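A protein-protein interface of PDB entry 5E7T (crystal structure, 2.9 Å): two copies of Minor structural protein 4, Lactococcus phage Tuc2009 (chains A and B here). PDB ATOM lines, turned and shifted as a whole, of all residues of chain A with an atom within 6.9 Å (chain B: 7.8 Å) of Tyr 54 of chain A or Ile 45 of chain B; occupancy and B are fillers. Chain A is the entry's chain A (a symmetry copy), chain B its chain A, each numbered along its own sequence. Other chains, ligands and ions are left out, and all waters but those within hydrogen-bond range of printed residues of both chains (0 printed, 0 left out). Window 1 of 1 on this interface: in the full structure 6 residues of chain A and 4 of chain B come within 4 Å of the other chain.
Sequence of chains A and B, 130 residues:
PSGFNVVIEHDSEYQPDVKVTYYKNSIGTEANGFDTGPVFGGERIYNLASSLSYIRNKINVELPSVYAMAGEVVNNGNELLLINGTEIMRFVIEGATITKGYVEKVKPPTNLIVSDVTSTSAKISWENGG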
ATOM      1  N   HIS A  10       6.354 -37.945 -36.884  1.00  0.00           N
ATOM      2  CA  HIS A  10       5.897 -37.626 -38.241  1.00  0.00           C
ATOM      3  C   HIS A  10       6.807 -36.646 -39.010  1.00  0.00           C
ATOM      4  O   HIS A  10       7.823 -36.183 -38.484  1.00  0.00           O
ATOM      5  CB  HIS A  10       4.464 -37.091 -38.178  1.00  0.00           C
ATOM      6  CG  HIS A  10       4.368 -35.826 -37.383  1.00  0.00           C
ATOM      7  ND1 HIS A  10       4.309 -35.842 -36.004  1.00  0.00           N
ATOM      8  CD2 HIS A  10       4.391 -34.548 -37.804  1.00  0.00           C
ATOM      9  CE1 HIS A  10       4.295 -34.578 -35.636  1.00  0.00           C
ATOM     10  NE2 HIS A  10       4.357 -33.767 -36.685  1.00  0.00           N
ATOM     11  N   TYR A  14       4.228 -29.124 -38.084  1.00  0.00           N
ATOM     12  CA  TYR A  14       3.088 -28.631 -37.334  1.00  0.00           C
ATOM     13  C   TYR A  14       2.528 -29.686 -36.320  1.00  0.00           C
ATOM     14  O   TYR A  14       3.280 -30.537 -35.817  1.00  0.00           O
ATOM     15  CB  TYR A  14       2.042 -28.079 -38.325  1.00  0.00           C
ATOM     16  CG  TYR A  14       2.549 -26.908 -39.154  1.00  0.00           C
ATOM     17  CD1 TYR A  14       2.431 -25.596 -38.697  1.00  0.00           C
ATOM     18  CD2 TYR A  14       3.141 -27.109 -40.398  1.00  0.00           C
ATOM     19  CE1 TYR A  14       2.902 -24.518 -39.451  1.00  0.00           C
ATOM     20  CE2 TYR A  14       3.607 -26.036 -41.161  1.00  0.00           C
ATOM     21  CZ  TYR A  14       3.493 -24.747 -40.678  1.00  0.00           C
ATOM     22  OH  TYR A  14       3.969 -23.700 -41.425  1.00  0.00           O
ATOM     23  N   GLN A  15       1.237 -29.579 -35.987  1.00  0.00           N
ATOM     24  CA  GLN A  15       0.552 -30.368 -34.985  1.00  0.00           C
ATOM     25  C   GLN A  15      -0.557 -31.254 -35.587  1.00  0.00           C
ATOM     26  O   GLN A  15      -1.734 -30.911 -35.415  1.00  0.00           O
ATOM     27  CB  GLN A  15      -0.049 -29.417 -33.947  1.00  0.00           C
ATOM     28  CG  GLN A  15       0.963 -28.698 -33.083  1.00  0.00           C
ATOM     29  CD  GLN A  15       1.599 -27.514 -33.751  1.00  0.00           C
ATOM     30  OE1 GLN A  15       0.923 -26.643 -34.330  1.00  0.00           O
ATOM     31  NE2 GLN A  15       2.931 -27.489 -33.688  1.00  0.00           N
ATOM     32  N   PRO A  16      -0.215 -32.427 -36.212  1.00  0.00           N
ATOM     33  CA  PRO A  16      -1.247 -33.275 -36.838  1.00  0.00           C
ATOM     34  C   PRO A  16      -2.259 -33.833 -35.874  1.00  0.00           C
ATOM     35  O   PRO A  16      -1.922 -34.166 -34.754  1.00  0.00           O
ATOM     36  CB  PRO A  16      -0.439 -34.409 -37.480  1.00  0.00           C
ATOM     37  CG  PRO A  16       0.864 -33.847 -37.702  1.00  0.00           C
ATOM     38  CD  PRO A  16       1.118 -32.971 -36.496  1.00  0.00           C
ATOM     39  N   ASP A  17      -3.494 -33.954 -36.315  1.00  0.00           N
ATOM     40  CA  ASP A  17      -4.495 -34.509 -35.436  1.00  0.00           C
ATOM     41  C   ASP A  17      -4.380 -36.024 -35.431  1.00  0.00           C
ATOM     42  O   ASP A  17      -3.892 -36.613 -36.403  1.00  0.00           O
ATOM     43  CB  ASP A  17      -5.888 -34.036 -35.846  1.00  0.00           C
ATOM     44  CG  ASP A  17      -6.998 -34.410 -34.885  1.00  0.00           C
ATOM     45  OD1 ASP A  17      -6.738 -34.440 -33.647  1.00  0.00           O
ATOM     46  OD2 ASP A  17      -8.140 -34.631 -35.360  1.00  0.00           O
ATOM     47  N   VAL A  18      -4.775 -36.653 -34.309  1.00  0.00           N
ATOM     48  CA  VAL A  18      -4.782 -38.108 -34.152  1.00  0.00           C
ATOM     49  C   VAL A  18      -6.124 -38.532 -33.644  1.00  0.00           C
ATOM     50  O   VAL A  18      -6.657 -37.903 -32.729  1.00  0.00           O
ATOM     51  CB  VAL A  18      -3.629 -38.684 -33.298  1.00  0.00           C
ATOM     52  CG1 VAL A  18      -3.789 -40.187 -33.123  1.00  0.00           C
ATOM     53  CG2 VAL A  18      -2.272 -38.387 -33.934  1.00  0.00           C
ATOM     54  N   LEU A  52      -3.831 -34.997 -26.572  1.00  0.00           N
ATOM     55  CA  LEU A  52      -2.655 -34.846 -27.426  1.00  0.00           C
ATOM     56  C   LEU A  52      -1.803 -33.630 -27.060  1.00  0.00           C
ATOM     57  O   LEU A  52      -2.333 -32.575 -26.731  1.00  0.00           O
ATOM     58  CB  LEU A  52      -3.084 -34.702 -28.899  1.00  0.00           C
ATOM     59  CG  LEU A  52      -4.105 -35.665 -29.504  1.00  0.00           C
ATOM     60  CD1 LEU A  52      -4.459 -35.233 -30.889  1.00  0.00           C
ATOM     61  CD2 LEU A  52      -3.596 -37.095 -29.522  1.00  0.00           C
ATOM     62  N   SER A  53      -0.477 -33.782 -27.149  1.00  0.00           N
ATOM     63  CA  SER A  53       0.521 -32.732 -26.919  1.00  0.00           C
ATOM     64  C   SER A  53       1.599 -32.943 -27.956  1.00  0.00           C
ATOM     65  O   SER A  53       1.792 -34.076 -28.397  1.00  0.00           O
ATOM     66  CB  SER A  53       1.096 -32.780 -25.514  1.00  0.00           C
ATOM     67  OG  SER A  53       1.752 -34.009 -25.285  1.00  0.00           O
ATOM     68  N   TYR A  54       2.274 -31.850 -28.368  1.00  0.00           N
ATOM     69  CA  TYR A  54       3.205 -31.836 -29.482  1.00  0.00           C
ATOM     70  C   TYR A  54       4.504 -31.146 -29.261  1.00  0.00           C
ATOM     71  O   TYR A  54       4.554 -30.080 -28.648  1.00  0.00           O
ATOM     72  CB  TYR A  54       2.544 -31.091 -30.661  1.00  0.00           C
ATOM     73  CG  TYR A  54       1.201 -31.628 -31.103  1.00  0.00           C
ATOM     74  CD1 TYR A  54       1.110 -32.607 -32.084  1.00  0.00           C
ATOM     75  CD2 TYR A  54       0.022 -31.154 -30.544  1.00  0.00           C
ATOM     76  CE1 TYR A  54      -0.123 -33.117 -32.488  1.00  0.00           C
ATOM     77  CE2 TYR A  54      -1.214 -31.680 -30.916  1.00  0.00           C
ATOM     78  CZ  TYR A  54      -1.278 -32.661 -31.892  1.00  0.00           C
ATOM     79  OH  TYR A  54      -2.478 -33.148 -32.316  1.00  0.00           O
ATOM     80  N   ILE A  55       5.555 -31.716 -29.861  1.00  0.00           N
ATOM     81  CA  ILE A  55       6.898 -31.146 -30.037  1.00  0.00           C
ATOM     82  C   ILE A  55       7.235 -31.368 -31.525  1.00  0.00           C
ATOM     83  O   ILE A  55       6.566 -32.177 -32.186  1.00  0.00           O
ATOM     84  CB  ILE A  55       8.024 -31.622 -29.076  1.00  0.00           C
ATOM     85  CG1 ILE A  55       8.399 -33.096 -29.316  1.00  0.00           C
ATOM     86  CG2 ILE A  55       7.674 -31.323 -27.636  1.00  0.00           C
ATOM     87  CD1 ILE A  55       9.510 -33.578 -28.538  1.00  0.00           C
ATOM     88  N   ARG A  56       8.247 -30.678 -32.049  1.00  0.00           N
ATOM     89  CA  ARG A  56       8.582 -30.816 -33.459  1.00  0.00           C
ATOM     90  C   ARG A  56       8.708 -32.270 -33.874  1.00  0.00           C
ATOM     91  O   ARG A  56       9.509 -32.994 -33.305  1.00  0.00           O
ATOM     92  CB  ARG A  56       9.839 -30.001 -33.812  1.00  0.00           C
ATOM     93  CG  ARG A  56      10.321 -30.196 -35.232  1.00  0.00           C
ATOM     94  CD  ARG A  56      11.542 -29.394 -35.549  1.00  0.00           C
ATOM     95  NE  ARG A  56      11.820 -29.469 -36.981  1.00  0.00           N
ATOM     96  CZ  ARG A  56      12.951 -29.919 -37.507  1.00  0.00           C
ATOM     97  NH1 ARG A  56      13.941 -30.324 -36.722  1.00  0.00           N
ATOM     98  NH2 ARG A  56      13.109 -29.953 -38.824  1.00  0.00           N
ATOM     99  N   ASN A  57       7.886 -32.702 -34.817  1.00  0.00           N
ATOM    100  CA  ASN A  57       7.922 -34.054 -35.358  1.00  0.00           C
ATOM    101  C   ASN A  57       7.458 -35.170 -34.420  1.00  0.00           C
ATOM    102  O   ASN A  57       7.455 -36.310 -34.866  1.00  0.00           O
ATOM    103  CB  ASN A  57       9.326 -34.393 -35.894  1.00  0.00           C
ATOM    104  CG  ASN A  57       9.878 -33.480 -36.956  1.00  0.00           C
ATOM    105  OD1 ASN A  57       9.171 -33.023 -37.855  1.00  0.00           O
ATOM    106  ND2 ASN A  57      11.191 -33.285 -36.928  1.00  0.00           N
ATOM    107  N   LYS A  58       7.068 -34.884 -33.157  1.00  0.00           N
ATOM    108  CA  LYS A  58       6.617 -35.923 -32.212  1.00  0.00           C
ATOM    109  C   LYS A  58       5.315 -35.565 -31.491  1.00  0.00           C
ATOM    110  O   LYS A  58       5.286 -34.641 -30.654  1.00  0.00           O
ATOM    111  CB  LYS A  58       7.696 -36.242 -31.149  1.00  0.00           C
ATOM    112  CG  LYS A  58       9.025 -36.713 -31.670  1.00  0.00           C
ATOM    113  CD  LYS A  58       9.995 -37.060 -30.557  1.00  0.00           C
ATOM    114  CE  LYS A  58       9.730 -38.410 -29.953  1.00  0.00           C
ATOM    115  NZ  LYS A  58      10.679 -38.724 -28.857  1.00  0.00           N
ATOM    116  N   ILE A  59       4.251 -36.361 -31.774  1.00  0.00           N
ATOM    117  CA  ILE A  59       2.899 -36.294 -31.163  1.00  0.00           C
ATOM    118  C   ILE A  59       2.919 -37.276 -30.000  1.00  0.00           C
ATOM    119  O   ILE A  59       3.417 -38.387 -30.157  1.00  0.00           O
ATOM    120  CB  ILE A  59       1.761 -36.709 -32.166  1.00  0.00           C
ATOM    121  CG1 ILE A  59       1.848 -35.954 -33.516  1.00  0.00           C
ATOM    122  CG2 ILE A  59       0.359 -36.583 -31.529  1.00  0.00           C
ATOM    123  CD1 ILE A  59       0.840 -36.386 -34.575  1.00  0.00           C
ATOM    124  N   ASN A  60       2.381 -36.890 -28.849  1.00  0.00           N
ATOM    125  CA  ASN A  60       2.296 -37.795 -27.714  1.00  0.00           C
ATOM    126  C   ASN A  60       0.819 -37.971 -27.465  1.00  0.00           C
ATOM    127  O   ASN A  60       0.119 -37.002 -27.113  1.00  0.00           O
ATOM    128  CB  ASN A  60       3.022 -37.254 -26.496  1.00  0.00           C
ATOM    129  CG  ASN A  60       2.700 -38.005 -25.239  1.00  0.00           C
ATOM    130  OD1 ASN A  60       1.680 -37.774 -24.590  1.00  0.00           O
ATOM    131  ND2 ASN A  60       3.554 -38.922 -24.865  1.00  0.00           N
ATOM    132  N   VAL B  20      -8.828 -25.150 -28.159  1.00  0.00           N
ATOM    133  CA  VAL B  20      -7.904 -24.616 -27.172  1.00  0.00           C
ATOM    134  C   VAL B  20      -6.580 -25.398 -27.102  1.00  0.00           C
ATOM    135  O   VAL B  20      -6.569 -26.647 -27.034  1.00  0.00           O
ATOM    136  CB  VAL B  20      -8.556 -24.473 -25.773  1.00  0.00           C
ATOM    137  CG1 VAL B  20      -7.687 -23.642 -24.836  1.00  0.00           C
ATOM    138  CG2 VAL B  20      -9.954 -23.866 -25.872  1.00  0.00           C
ATOM    139  N   THR B  21      -5.471 -24.632 -27.125  1.00  0.00           N
ATOM    140  CA  THR B  21      -4.104 -25.096 -26.927  1.00  0.00           C
ATOM    141  C   THR B  21      -3.429 -24.221 -25.863  1.00  0.00           C
ATOM    142  O   THR B  21      -3.834 -23.072 -25.622  1.00  0.00           O
ATOM    143  CB  THR B  21      -3.248 -25.139 -28.214  1.00  0.00           C
ATOM    144  OG1 THR B  21      -3.211 -23.856 -28.837  1.00  0.00           O
ATOM    145  CG2 THR B  21      -3.665 -26.221 -29.174  1.00  0.00           C
ATOM    146  N   TYR B  22      -2.394 -24.782 -25.244  1.00  0.00           N
ATOM    147  CA  TYR B  22      -1.573 -24.149 -24.234  1.00  0.00           C
ATOM    148  C   TYR B  22      -0.096 -24.403 -24.593  1.00  0.00           C
ATOM    149  O   TYR B  22       0.277 -25.514 -24.979  1.00  0.00           O
ATOM    150  CB  TYR B  22      -1.912 -24.716 -22.832  1.00  0.00           C
ATOM    151  CG  TYR B  22      -0.933 -24.272 -21.757  1.00  0.00           C
ATOM    152  CD1 TYR B  22       0.243 -24.980 -21.519  1.00  0.00           C
ATOM    153  CD2 TYR B  22      -1.187 -23.148 -20.976  1.00  0.00           C
ATOM    154  CE1 TYR B  22       1.156 -24.566 -20.548  1.00  0.00           C
ATOM    155  CE2 TYR B  22      -0.292 -22.736 -19.989  1.00  0.00           C
ATOM    156  CZ  TYR B  22       0.887 -23.436 -19.792  1.00  0.00           C
ATOM    157  OH  TYR B  22       1.789 -23.029 -18.842  1.00  0.00           O
ATOM    158  N   TYR B  23       0.745 -23.387 -24.418  1.00  0.00           N
ATOM    159  CA  TYR B  23       2.178 -23.472 -24.693  1.00  0.00           C
ATOM    160  C   TYR B  23       2.960 -22.342 -24.032  1.00  0.00           C
ATOM    161  O   TYR B  23       2.446 -21.225 -23.870  1.00  0.00           O
ATOM    162  CB  TYR B  23       2.472 -23.548 -26.196  1.00  0.00           C
ATOM    163  CG  TYR B  23       1.807 -22.469 -27.019  1.00  0.00           C
ATOM    164  CD1 TYR B  23       0.550 -22.667 -27.578  1.00  0.00           C
ATOM    165  CD2 TYR B  23       2.446 -21.259 -27.259  1.00  0.00           C
ATOM    166  CE1 TYR B  23      -0.075 -21.668 -28.316  1.00  0.00           C
ATOM    167  CE2 TYR B  23       1.828 -20.252 -28.000  1.00  0.00           C
ATOM    168  CZ  TYR B  23       0.578 -20.472 -28.548  1.00  0.00           C
ATOM    169  OH  TYR B  23      -0.012 -19.491 -29.307  1.00  0.00           O
ATOM    170  N   LYS B  24       4.200 -22.660 -23.630  1.00  0.00           N
ATOM    171  CA  LYS B  24       5.126 -21.757 -22.968  1.00  0.00           C
ATOM    172  C   LYS B  24       6.242 -21.335 -23.911  1.00  0.00           C
ATOM    173  O   LYS B  24       6.732 -22.149 -24.697  1.00  0.00           O
ATOM    174  CB  LYS B  24       5.778 -22.502 -21.806  1.00  0.00           C
ATOM    175  CG  LYS B  24       5.149 -22.239 -20.473  1.00  0.00           C
ATOM    176  CD  LYS B  24       5.475 -23.312 -19.459  1.00  0.00           C
ATOM    177  CE  LYS B  24       6.865 -23.294 -18.896  1.00  0.00           C
ATOM    178  NZ  LYS B  24       6.857 -23.632 -17.449  1.00  0.00           N
ATOM    179  N   SER B  26       6.630 -19.256 -26.531  1.00  0.00           N
ATOM    180  CA  SER B  26       6.433 -18.979 -27.961  1.00  0.00           C
ATOM    181  C   SER B  26       7.134 -17.608 -28.251  1.00  0.00           C
ATOM    182  O   SER B  26       7.476 -16.903 -27.301  1.00  0.00           O
ATOM    183  CB  SER B  26       4.946 -18.868 -28.264  1.00  0.00           C
ATOM    184  OG  SER B  26       4.293 -18.043 -27.311  1.00  0.00           O
ATOM    185  N   GLY B  41      10.653 -20.888 -30.451  1.00  0.00           N
ATOM    186  CA  GLY B  41       9.390 -21.063 -31.167  1.00  0.00           C
ATOM    187  C   GLY B  41       8.280 -21.558 -30.278  1.00  0.00           C
ATOM    188  O   GLY B  41       7.112 -21.417 -30.621  1.00  0.00           O
ATOM    189  N   GLY B  42       8.647 -22.134 -29.137  1.00  0.00           N
ATOM    190  CA  GLY B  42       7.678 -22.616 -28.168  1.00  0.00           C
ATOM    191  C   GLY B  42       7.911 -24.033 -27.712  1.00  0.00           C
ATOM    192  O   GLY B  42       8.301 -24.884 -28.509  1.00  0.00           O
ATOM    193  N   GLU B  43       7.654 -24.296 -26.424  1.00  0.00           N
ATOM    194  CA  GLU B  43       7.810 -25.607 -25.800  1.00  0.00           C
ATOM    195  C   GLU B  43       6.605 -26.474 -26.198  1.00  0.00           C
ATOM    196  O   GLU B  43       5.916 -26.142 -27.164  1.00  0.00           O
ATOM    197  CB  GLU B  43       7.897 -25.458 -24.272  1.00  0.00           C
ATOM    198  CG  GLU B  43       9.227 -24.969 -23.735  1.00  0.00           C
ATOM    199  CD  GLU B  43       9.260 -24.836 -22.219  1.00  0.00           C
ATOM    200  OE1 GLU B  43       8.879 -25.797 -21.508  1.00  0.00           O
ATOM    201  OE2 GLU B  43       9.674 -23.755 -21.740  1.00  0.00           O
ATOM    202  N   ARG B  44       6.354 -27.586 -25.475  1.00  0.00           N
ATOM    203  CA  ARG B  44       5.242 -28.493 -25.767  1.00  0.00           C
ATOM    204  C   ARG B  44       3.903 -27.729 -25.825  1.00  0.00           C
ATOM    205  O   ARG B  44       3.656 -26.848 -24.993  1.00  0.00           O
ATOM    206  CB  ARG B  44       5.209 -29.653 -24.757  1.00  0.00           C
ATOM    207  CG  ARG B  44       4.210 -30.760 -25.070  1.00  0.00           C
ATOM    208  CD  ARG B  44       4.335 -31.991 -24.173  1.00  0.00           C
ATOM    209  NE  ARG B  44       5.585 -32.715 -24.426  1.00  0.00           N
ATOM    210  CZ  ARG B  44       5.755 -33.653 -25.351  1.00  0.00           C
ATOM    211  NH1 ARG B  44       4.744 -34.023 -26.128  1.00  0.00           N
ATOM    212  NH2 ARG B  44       6.936 -34.229 -25.507  1.00  0.00           N
ATOM    213  N   ILE B  45       3.118 -27.997 -26.896  1.00  0.00           N
ATOM    214  CA  ILE B  45       1.776 -27.471 -27.154  1.00  0.00           C
ATOM    215  C   ILE B  45       0.844 -28.550 -26.646  1.00  0.00           C
ATOM    216  O   ILE B  45       0.983 -29.707 -27.027  1.00  0.00           O
ATOM    217  CB  ILE B  45       1.530 -27.222 -28.657  1.00  0.00           C
ATOM    218  CG1 ILE B  45       2.410 -26.079 -29.179  1.00  0.00           C
ATOM    219  CG2 ILE B  45       0.046 -26.969 -28.932  1.00  0.00           C
ATOM    220  CD1 ILE B  45       2.451 -25.960 -30.603  1.00  0.00           C
ATOM    221  N   TYR B  46      -0.063 -28.191 -25.750  1.00  0.00           N
ATOM    222  CA  TYR B  46      -1.016 -29.133 -25.183  1.00  0.00           C
ATOM    223  C   TYR B  46      -2.381 -28.755 -25.708  1.00  0.00           C
ATOM    224  O   TYR B  46      -2.716 -27.570 -25.735  1.00  0.00           O
ATOM    225  CB  TYR B  46      -1.034 -29.018 -23.651  1.00  0.00           C
ATOM    226  CG  TYR B  46       0.246 -29.424 -22.957  1.00  0.00           C
ATOM    227  CD1 TYR B  46       1.292 -28.518 -22.788  1.00  0.00           C
ATOM    228  CD2 TYR B  46       0.378 -30.686 -22.382  1.00  0.00           C
ATOM    229  CE1 TYR B  46       2.458 -28.875 -22.112  1.00  0.00           C
ATOM    230  CE2 TYR B  46       1.542 -31.058 -21.713  1.00  0.00           C
ATOM    231  CZ  TYR B  46       2.576 -30.146 -21.568  1.00  0.00           C
ATOM    232  OH  TYR B  46       3.719 -30.524 -20.899  1.00  0.00           O
ATOM    233  N   ASN B  47      -3.178 -29.742 -26.107  1.00  0.00           N
ATOM    234  CA  ASN B  47      -4.552 -29.497 -26.516  1.00  0.00           C
ATOM    235  C   ASN B  47      -5.359 -29.485 -25.211  1.00  0.00           C
ATOM    236  O   ASN B  47      -5.270 -30.454 -24.442  1.00  0.00           O
ATOM    237  CB  ASN B  47      -5.061 -30.629 -27.409  1.00  0.00           C
ATOM    238  CG  ASN B  47      -4.640 -30.614 -28.841  1.00  0.00           C
ATOM    239  OD1 ASN B  47      -3.866 -29.766 -29.314  1.00  0.00           O
ATOM    240  ND2 ASN B  47      -5.163 -31.585 -29.560  1.00  0.00           N
ATOM    241  N   LEU B  48      -6.118 -28.408 -24.951  1.00  0.00           N
ATOM    242  CA  LEU B  48      -6.936 -28.323 -23.740  1.00  0.00           C
ATOM    243  C   LEU B  48      -8.374 -28.754 -24.003  1.00  0.00           C
ATOM    244  O   LEU B  48      -9.000 -28.279 -24.943  1.00  0.00           O
ATOM    245  CB  LEU B  48      -6.896 -26.925 -23.096  1.00  0.00           C
ATOM    246  CG  LEU B  48      -5.528 -26.425 -22.640  1.00  0.00           C
ATOM    247  CD1 LEU B  48      -5.663 -25.157 -21.826  1.00  0.00           C
ATOM    248  CD2 LEU B  48      -4.723 -27.520 -21.900  1.00  0.00           C
ATOM    249  N   ARG B  90      -4.296 -20.381 -26.196  1.00  0.00           N
ATOM    250  CA  ARG B  90      -4.737 -19.993 -27.521  1.00  0.00           C
ATOM    251  C   ARG B  90      -6.114 -20.600 -27.812  1.00  0.00           C
ATOM    252  O   ARG B  90      -6.312 -21.795 -27.586  1.00  0.00           O
ATOM    253  CB  ARG B  90      -3.686 -20.482 -28.524  1.00  0.00           C
ATOM    254  CG  ARG B  90      -3.858 -19.917 -29.904  1.00  0.00           C
ATOM    255  CD  ARG B  90      -3.254 -20.808 -30.961  1.00  0.00           C
ATOM    256  NE  ARG B  90      -3.453 -20.200 -32.269  1.00  0.00           N
ATOM    257  CZ  ARG B  90      -3.301 -20.817 -33.432  1.00  0.00           C
ATOM    258  NH1 ARG B  90      -2.973 -22.093 -33.472  1.00  0.00           N
ATOM    259  NH2 ARG B  90      -3.521 -20.165 -34.567  1.00  0.00           N
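Ile 45 of chain B touches Gln 15 of chain A (CD1 to NE2, 3.5 Å). O of Leu 52 of chain A touches C of Tyr 46 of chain B, at 3.95 Å. Ser 53 of chain A touches Ile 45 of chain B (CA to O, 3.1 Å). Ser 53 of chain A touches Tyr 46 of chain B. CA of Arg 44 of chain B touches O of Tyr 54 of chain A, 3.4 Å away. OD1 of Asn 47 of chain B touches CE2 of Tyr 54 of chain A (3.6 Å). CG2 of Ile 55 of chain A touches NH2 of Arg 44 of chain B, 3.7 Å away. Asn 60 of chain A touches Arg 44 of chain B.
No position is printed for both chains. Of the 11 pairs that touch across the chains among the printed residues, none has its exchanged pair printed and touching as well.
Of chain B, only Arg 44, Ile 45 and Asn 47 come within 4 Å of Tyr 54 of chain A. Ile 45 of chain B touches three residues of chain A. Of the printed residues of chain B, Asn 60 of chain A touches Arg 44. Printed residues of chain A within 4 Å of Arg 44 of chain B: Ser 53 (3.1 Å), Tyr 54 (3.4 Å), Ile 55 (3.7 Å) and Asn 60 (3.7 Å). Printed residues of chain A within 4 Å of Asn 47 of chain B: Leu 52 (3.0 Å) and Tyr 54 (3.6 Å). Of the printed residues of chain B, Ile 55 of chain A touches Arg 44. Of the printed residues of chain B, Leu 52 of chain A touches Tyr 46 and Asn 47. The nearest residue of chain A that does not touch Ile 45 of chain B is Leu 52 of chain A (4.4 Å). The nearest printed residue of chain B that does not touch Asn 60 of chain A is Tyr 46 of chain B (7.3 Å).
The backbone carbonyl oxygen of Pro 16 of chain A is in hydrogen-bond range of the side-chain hydroxyl of Tyr 54 of chain A (2.7 Å). The backbone NH of Asn 60 of chain A lies within hydrogen-bond range of the backbone carbonyl oxygen of Ser 53 of chain A, at 2.9 Å. The backbone carbonyl oxygen of Tyr 22 of chain B lies within hydrogen-bond range of the backbone NH of Tyr 46 of chain B (2.8 Å).
The backbone NH of Asn 47 of chain B lies within hydrogen-bond range of the backbone carbonyl oxygen of Leu 52 of chain A (3.0 Å). The backbone NH of Tyr 54 of chain A sits at hydrogen-bond distance from the backbone carbonyl oxygen of Ile 45 of chain B (2.8 Å). The guanidinium group (NH1) of Arg 44 of chain B is in hydrogen-bond range of the side-chain hydroxyl (OG) of Ser 53 of chain A (3.1 Å).
Of the 15 printed residues of chain B, 4 touch a printed residue of chain A. Hydrophobic or aromatic side chains of chain B that line the printed part of chain A: Ile 45 and Tyr 46. Among the printed residues, 11 pairs touch across the chains.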
